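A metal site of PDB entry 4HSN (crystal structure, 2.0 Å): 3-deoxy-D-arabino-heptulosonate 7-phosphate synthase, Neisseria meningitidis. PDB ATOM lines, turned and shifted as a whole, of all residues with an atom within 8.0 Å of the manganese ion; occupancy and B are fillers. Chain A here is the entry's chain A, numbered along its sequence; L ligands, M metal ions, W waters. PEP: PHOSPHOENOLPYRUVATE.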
ATOM      1  N   GLY A  61     -37.377   8.202   8.053  1.00  0.00           N
ATOM      2  CA  GLY A  61     -37.211   7.123   9.013  1.00  0.00           C
ATOM      3  C   GLY A  61     -35.747   6.776   9.230  1.00  0.00           C
ATOM      4  O   GLY A  61     -34.868   7.521   8.868  1.00  0.00           O
ATOM      5  N   PRO A  62     -35.503   5.689   9.953  1.00  0.00           N
ATOM      6  CA  PRO A  62     -34.106   5.238  10.308  1.00  0.00           C
ATOM      7  C   PRO A  62     -33.139   5.086   9.149  1.00  0.00           C
ATOM      8  O   PRO A  62     -33.561   4.822   8.042  1.00  0.00           O
ATOM      9  CB  PRO A  62     -34.360   3.940  11.046  1.00  0.00           C
ATOM     10  CG  PRO A  62     -35.683   4.055  11.638  1.00  0.00           C
ATOM     11  CD  PRO A  62     -36.496   4.799  10.535  1.00  0.00           C
ATOM     12  N   CYS A  63     -31.881   5.380   9.385  1.00  0.00           N
ATOM     13  CA  CYS A  63     -30.875   5.090   8.417  1.00  0.00           C
ATOM     14  C   CYS A  63     -31.035   3.533   8.121  1.00  0.00           C
ATOM     15  O   CYS A  63     -31.083   3.148   6.957  1.00  0.00           O
ATOM     16  CB  CYS A  63     -29.520   5.394   9.010  1.00  0.00           C
ATOM     17  SG  CYS A  63     -28.106   4.875   7.985  1.00  0.00           S
ATOM     18  N   SER A  64     -31.134   2.747   9.166  1.00  0.00           N
ATOM     19  CA  SER A  64     -31.241   1.325   9.035  1.00  0.00           C
ATOM     20  C   SER A  64     -32.164   0.761  10.086  1.00  0.00           C
ATOM     21  O   SER A  64     -32.269   1.304  11.186  1.00  0.00           O
ATOM     22  CB  SER A  64     -29.877   0.713   9.231  1.00  0.00           C
ATOM     23  OG  SER A  64     -29.313   1.000  10.516  1.00  0.00           O
ATOM     24  N   ARG A  94     -38.910   5.059   5.796  1.00  0.00           N
ATOM     25  CA  ARG A  94     -37.647   4.411   5.440  1.00  0.00           C
ATOM     26  C   ARG A  94     -37.558   3.114   6.230  1.00  0.00           C
ATOM     27  O   ARG A  94     -37.552   3.131   7.486  1.00  0.00           O
ATOM     28  CB  ARG A  94     -36.402   5.218   5.868  1.00  0.00           C
ATOM     29  CG  ARG A  94     -36.108   6.443   4.996  1.00  0.00           C
ATOM     30  CD  ARG A  94     -34.868   7.193   5.453  1.00  0.00           C
ATOM     31  NE  ARG A  94     -33.733   6.299   5.565  1.00  0.00           N
ATOM     32  CZ  ARG A  94     -32.643   6.241   4.806  1.00  0.00           C
ATOM     33  NH1 ARG A  94     -32.488   6.968   3.770  1.00  0.00           N
ATOM     34  NH2 ARG A  94     -31.729   5.294   5.066  1.00  0.00           N
ATOM     35  N   TYR A  96     -34.962   0.324   5.687  1.00  0.00           N
ATOM     36  CA  TYR A  96     -33.788  -0.060   4.955  1.00  0.00           C
ATOM     37  C   TYR A  96     -33.126  -1.270   5.614  1.00  0.00           C
ATOM     38  O   TYR A  96     -32.717  -1.166   6.769  1.00  0.00           O
ATOM     39  CB  TYR A  96     -32.842   1.111   4.937  1.00  0.00           C
ATOM     40  CG  TYR A  96     -33.113   2.119   3.853  1.00  0.00           C
ATOM     41  CD1 TYR A  96     -34.378   2.669   3.661  1.00  0.00           C
ATOM     42  CD2 TYR A  96     -32.107   2.584   3.055  1.00  0.00           C
ATOM     43  CE1 TYR A  96     -34.623   3.620   2.651  1.00  0.00           C
ATOM     44  CE2 TYR A  96     -32.289   3.598   2.104  1.00  0.00           C
ATOM     45  CZ  TYR A  96     -33.567   4.106   1.921  1.00  0.00           C
ATOM     46  OH  TYR A  96     -33.762   5.053   0.896  1.00  0.00           O
ATOM     47  N   LYS A  99     -27.395  -2.168   3.799  1.00  0.00           N
ATOM     48  CA  LYS A  99     -26.532  -0.998   3.955  1.00  0.00           C
ATOM     49  C   LYS A  99     -25.246  -1.228   3.219  1.00  0.00           C
ATOM     50  O   LYS A  99     -24.510  -2.149   3.525  1.00  0.00           O
ATOM     51  CB  LYS A  99     -26.251  -0.707   5.449  1.00  0.00           C
ATOM     52  CG  LYS A  99     -27.503  -0.593   6.308  1.00  0.00           C
ATOM     53  CD  LYS A  99     -28.505   0.446   5.708  1.00  0.00           C
ATOM     54  CE  LYS A  99     -27.855   1.870   5.771  1.00  0.00           C
ATOM     55  NZ  LYS A  99     -28.740   2.852   5.063  1.00  0.00           N
ATOM     56  N   PRO A 100     -24.881  -0.282   2.322  1.00  0.00           N
ATOM     57  CA  PRO A 100     -23.614  -0.375   1.665  1.00  0.00           C
ATOM     58  C   PRO A 100     -22.574   0.253   2.561  1.00  0.00           C
ATOM     59  O   PRO A 100     -22.785   1.362   3.052  1.00  0.00           O
ATOM     60  CB  PRO A 100     -23.829   0.474   0.397  1.00  0.00           C
ATOM     61  CG  PRO A 100     -24.869   1.504   0.782  1.00  0.00           C
ATOM     62  CD  PRO A 100     -25.750   0.797   1.783  1.00  0.00           C
ATOM     63  N   GLU A 145     -33.678   0.684   0.184  1.00  0.00           N
ATOM     64  CA  GLU A 145     -32.678   0.608  -0.817  1.00  0.00           C
ATOM     65  C   GLU A 145     -32.548  -0.751  -1.329  1.00  0.00           C
ATOM     66  O   GLU A 145     -32.380  -1.676  -0.535  1.00  0.00           O
ATOM     67  CB  GLU A 145     -31.319   1.072  -0.338  1.00  0.00           C
ATOM     68  CG  GLU A 145     -30.208   0.967  -1.417  1.00  0.00           C
ATOM     69  CD  GLU A 145     -28.789   1.401  -1.053  1.00  0.00           C
ATOM     70  OE1 GLU A 145     -28.614   2.227  -0.091  1.00  0.00           O
ATOM     71  OE2 GLU A 145     -27.841   0.984  -1.825  1.00  0.00           O
ATOM     72  N   ARG A 167     -23.543   4.718  -4.431  1.00  0.00           N
ATOM     73  CA  ARG A 167     -22.446   3.866  -4.765  1.00  0.00           C
ATOM     74  C   ARG A 167     -22.796   2.887  -5.887  1.00  0.00           C
ATOM     75  O   ARG A 167     -21.931   2.178  -6.348  1.00  0.00           O
ATOM     76  CB  ARG A 167     -21.971   3.106  -3.513  1.00  0.00           C
ATOM     77  CG  ARG A 167     -21.371   4.056  -2.472  1.00  0.00           C
ATOM     78  CD  ARG A 167     -21.107   3.396  -1.110  1.00  0.00           C
ATOM     79  NE  ARG A 167     -20.772   4.393  -0.097  1.00  0.00           N
ATOM     80  CZ  ARG A 167     -21.610   5.268   0.470  1.00  0.00           C
ATOM     81  NH1 ARG A 167     -22.886   5.351   0.149  1.00  0.00           N
ATOM     82  NH2 ARG A 167     -21.146   6.181   1.314  1.00  0.00           N
ATOM     83  N   LYS A 188     -29.667   8.074  -6.639  1.00  0.00           N
ATOM     84  CA  LYS A 188     -28.846   9.094  -6.017  1.00  0.00           C
ATOM     85  C   LYS A 188     -27.698   9.481  -6.867  1.00  0.00           C
ATOM     86  O   LYS A 188     -27.130   8.650  -7.613  1.00  0.00           O
ATOM     87  CB  LYS A 188     -28.314   8.553  -4.682  1.00  0.00           C
ATOM     88  CG  LYS A 188     -29.441   8.373  -3.686  1.00  0.00           C
ATOM     89  CD  LYS A 188     -28.977   8.144  -2.292  1.00  0.00           C
ATOM     90  CE  LYS A 188     -29.925   8.905  -1.334  1.00  0.00           C
ATOM     91  NZ  LYS A 188     -29.400   8.688   0.052  1.00  0.00           N
ATOM     92  N   ASP A 267     -32.241  14.974  -0.589  1.00  0.00           N
ATOM     93  CA  ASP A 267     -31.883  14.247   0.688  1.00  0.00           C
ATOM     94  C   ASP A 267     -31.311  15.237   1.668  1.00  0.00           C
ATOM     95  O   ASP A 267     -30.347  15.932   1.323  1.00  0.00           O
ATOM     96  CB  ASP A 267     -30.836  13.172   0.362  1.00  0.00           C
ATOM     97  CG  ASP A 267     -30.479  12.290   1.586  1.00  0.00           C
ATOM     98  OD1 ASP A 267     -30.990  12.518   2.705  1.00  0.00           O
ATOM     99  OD2 ASP A 267     -29.728  11.323   1.360  1.00  0.00           O
ATOM    100  N   SER A 269     -29.997  14.489   4.393  1.00  0.00           N
ATOM    101  CA  SER A 269     -28.967  13.795   5.236  1.00  0.00           C
ATOM    102  C   SER A 269     -27.689  13.537   4.412  1.00  0.00           C
ATOM    103  O   SER A 269     -27.401  14.262   3.406  1.00  0.00           O
ATOM    104  CB  SER A 269     -29.537  12.518   5.865  1.00  0.00           C
ATOM    105  OG  SER A 269     -28.721  12.063   6.968  1.00  0.00           O
ATOM    106  N   HIS A 270     -26.867  12.569   4.892  1.00  0.00           N
ATOM    107  CA  HIS A 270     -25.677  12.210   4.157  1.00  0.00           C
ATOM    108  C   HIS A 270     -24.809  13.427   3.774  1.00  0.00           C
ATOM    109  O   HIS A 270     -24.450  14.231   4.658  1.00  0.00           O
ATOM    110  CB  HIS A 270     -26.049  11.283   2.976  1.00  0.00           C
ATOM    111  CG  HIS A 270     -26.853  10.103   3.433  1.00  0.00           C
ATOM    112  ND1 HIS A 270     -28.209   9.974   3.182  1.00  0.00           N
ATOM    113  CD2 HIS A 270     -26.510   9.024   4.211  1.00  0.00           C
ATOM    114  CE1 HIS A 270     -28.668   8.916   3.847  1.00  0.00           C
ATOM    115  NE2 HIS A 270     -27.649   8.327   4.437  1.00  0.00           N
ATOM    116  N   MET A 302     -35.895  13.533   1.586  1.00  0.00           N
ATOM    117  CA  MET A 302     -35.502  12.392   2.368  1.00  0.00           C
ATOM    118  C   MET A 302     -34.867  12.808   3.673  1.00  0.00           C
ATOM    119  O   MET A 302     -34.115  13.781   3.719  1.00  0.00           O
ATOM    120  CB  MET A 302     -34.623  11.444   1.485  1.00  0.00           C
ATOM    121  CG  MET A 302     -33.904  10.396   2.283  1.00  0.00           C
ATOM    122  SD  MET A 302     -32.822   9.242   1.296  1.00  0.00           S
ATOM    123  CE  MET A 302     -33.873   8.935  -0.100  1.00  0.00           C
ATOM    124  N   GLU A 304     -33.345  11.255   7.607  1.00  0.00           N
ATOM    125  CA  GLU A 304     -32.955  10.140   8.554  1.00  0.00           C
ATOM    126  C   GLU A 304     -33.295  10.533   9.989  1.00  0.00           C
ATOM    127  O   GLU A 304     -32.852  11.575  10.520  1.00  0.00           O
ATOM    128  CB  GLU A 304     -31.517   9.830   8.408  1.00  0.00           C
ATOM    129  CG  GLU A 304     -31.215   9.219   7.061  1.00  0.00           C
ATOM    130  CD  GLU A 304     -29.791   8.646   6.976  1.00  0.00           C
ATOM    131  OE1 GLU A 304     -28.814   9.354   7.320  1.00  0.00           O
ATOM    132  OE2 GLU A 304     -29.699   7.466   6.523  1.00  0.00           O
ATOM    133  N   SER A 321     -30.140   4.800  16.349  1.00  0.00           N
ATOM    134  CA  SER A 321     -29.353   4.297  15.235  1.00  0.00           C
ATOM    135  C   SER A 321     -28.014   3.675  15.597  1.00  0.00           C
ATOM    136  O   SER A 321     -27.328   4.195  16.412  1.00  0.00           O
ATOM    137  CB  SER A 321     -29.148   5.396  14.148  1.00  0.00           C
ATOM    138  OG  SER A 321     -28.434   4.845  13.002  1.00  0.00           O
ATOM    139  N   THR A 323     -26.296   2.922  12.727  1.00  0.00           N
ATOM    140  CA  THR A 323     -25.565   3.337  11.504  1.00  0.00           C
ATOM    141  C   THR A 323     -25.425   4.913  11.479  1.00  0.00           C
ATOM    142  O   THR A 323     -24.863   5.459  12.413  1.00  0.00           O
ATOM    143  CB  THR A 323     -26.180   2.727  10.177  1.00  0.00           C
ATOM    144  OG1 THR A 323     -27.610   2.926  10.124  1.00  0.00           O
ATOM    145  CG2 THR A 323     -25.820   1.186  10.100  1.00  0.00           C
ATOM    146  N   ASP A 324     -25.889   5.612  10.450  1.00  0.00           N
ATOM    147  CA  ASP A 324     -25.769   7.115  10.446  1.00  0.00           C
ATOM    148  C   ASP A 324     -26.626   7.684  11.589  1.00  0.00           C
ATOM    149  O   ASP A 324     -27.696   7.195  11.884  1.00  0.00           O
ATOM    150  CB  ASP A 324     -26.250   7.783   9.105  1.00  0.00           C
ATOM    151  CG  ASP A 324     -25.439   7.329   7.879  1.00  0.00           C
ATOM    152  OD1 ASP A 324     -24.317   6.913   8.029  1.00  0.00           O
ATOM    153  OD2 ASP A 324     -26.064   7.188   6.813  1.00  0.00           O
ATOM    154  N   ALA A 325     -26.218   8.831  12.144  1.00  0.00           N
ATOM    155  CA  ALA A 325     -26.956   9.488  13.198  1.00  0.00           C
ATOM    156  C   ALA A 325     -28.239  10.110  12.607  1.00  0.00           C
ATOM    157  O   ALA A 325     -28.247  10.563  11.495  1.00  0.00           O
ATOM    158  CB  ALA A 325     -26.064  10.565  13.850  1.00  0.00           C
ATOM    159  N   CYS A 326     -29.327  10.005  13.351  1.00  0.00           N
ATOM    160  CA  CYS A 326     -30.646  10.437  12.906  1.00  0.00           C
ATOM    161  C   CYS A 326     -31.127  11.580  13.841  1.00  0.00           C
ATOM    162  O   CYS A 326     -30.655  11.711  14.999  1.00  0.00           O
ATOM    163  CB  CYS A 326     -31.609   9.306  13.041  1.00  0.00           C
ATOM    164  SG  CYS A 326     -31.233   7.940  11.905  1.00  0.00           S
HETATM  165  C1  PEP L   1     -29.164   5.950   2.555  1.00  0.00           C
HETATM  166  O1  PEP L   1     -30.139   6.510   1.975  1.00  0.00           O
HETATM  167  O2' PEP L   1     -29.269   5.539   3.719  1.00  0.00           O
HETATM  168  C2  PEP L   1     -27.851   5.749   1.858  1.00  0.00           C
HETATM  169  C3  PEP L   1     -27.095   4.653   2.030  1.00  0.00           C
HETATM  170  O2  PEP L   1     -27.484   6.761   0.893  1.00  0.00           O
HETATM  171  P   PEP L   1     -26.151   7.161   0.119  1.00  0.00           P
HETATM  172  O1P PEP L   1     -26.321   6.145  -0.985  1.00  0.00           O
HETATM  173  O2P PEP L   1     -26.391   8.677  -0.060  1.00  0.00           O
HETATM  174  O3P PEP L   1     -24.994   7.043   1.071  1.00  0.00           O
HETATM  175 MN    MN M   1     -27.814   6.717   6.081  1.00  0.00          MN
HETATM  176  O   HOH W   1     -27.205   5.367   4.882  1.00  0.00           O
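The side-chain sulfur (SG) of Cys 326 lies within hydrogen-bond range of the backbone carbonyl oxygen (O) of Asp 324, 3.6 Å away.
The side-chain hydroxyl (OG) of Ser 321 sits at hydrogen-bond distance from the backbone carbonyl oxygen (O) of Asp 324.
The side-chain carboxylate (OE2) of Glu 304 lies close to the guanidinium group (NH2) of Arg 94.
OE1 of Glu 304 sits at hydrogen-bond distance from OG of Ser 269.
The backbone carbonyl oxygen of Cys 63 is in hydrogen-bond range of the side-chain amino group of Lys 99 (3.0 Å).
The guanidinium group (NH2) of Arg 94 sits at hydrogen-bond distance from the backbone carbonyl oxygen (O) of Cys 63 (2.9 Å).
The side-chain sulfur of Cys 63 sits close to the side-chain hydroxyl of Thr 323 (2.9 Å).
SG of Cys 326 lies within hydrogen-bond range of N of Cys 63 (3.7 Å).
NE2 of His 270 lies close to O2' of the ligand (3.3 Å).
NZ of Lys 99 is in salt-bridge range of O2' of the ligand (3.1 Å).
O2' of the ligand is in salt-bridge range of NH2 of Arg 94, at 2.8 Å.
An oxygen (O1) of the ligand is in salt-bridge range of the side-chain amino group of Lys 188 (3.0 Å).
NH1 of Arg 167 is in salt-bridge range of O3P of the ligand, 2.9 Å away.
The manganese ion is bound by water W1, the side-chain carboxylate (OD2) of Asp 324, the side-chain carboxylate (OE2) of Glu 304, a ring nitrogen (NE2) of His 270 and the side-chain sulfur (SG) of Cys 63.
The manganese ion has five donor atoms within binding distance.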
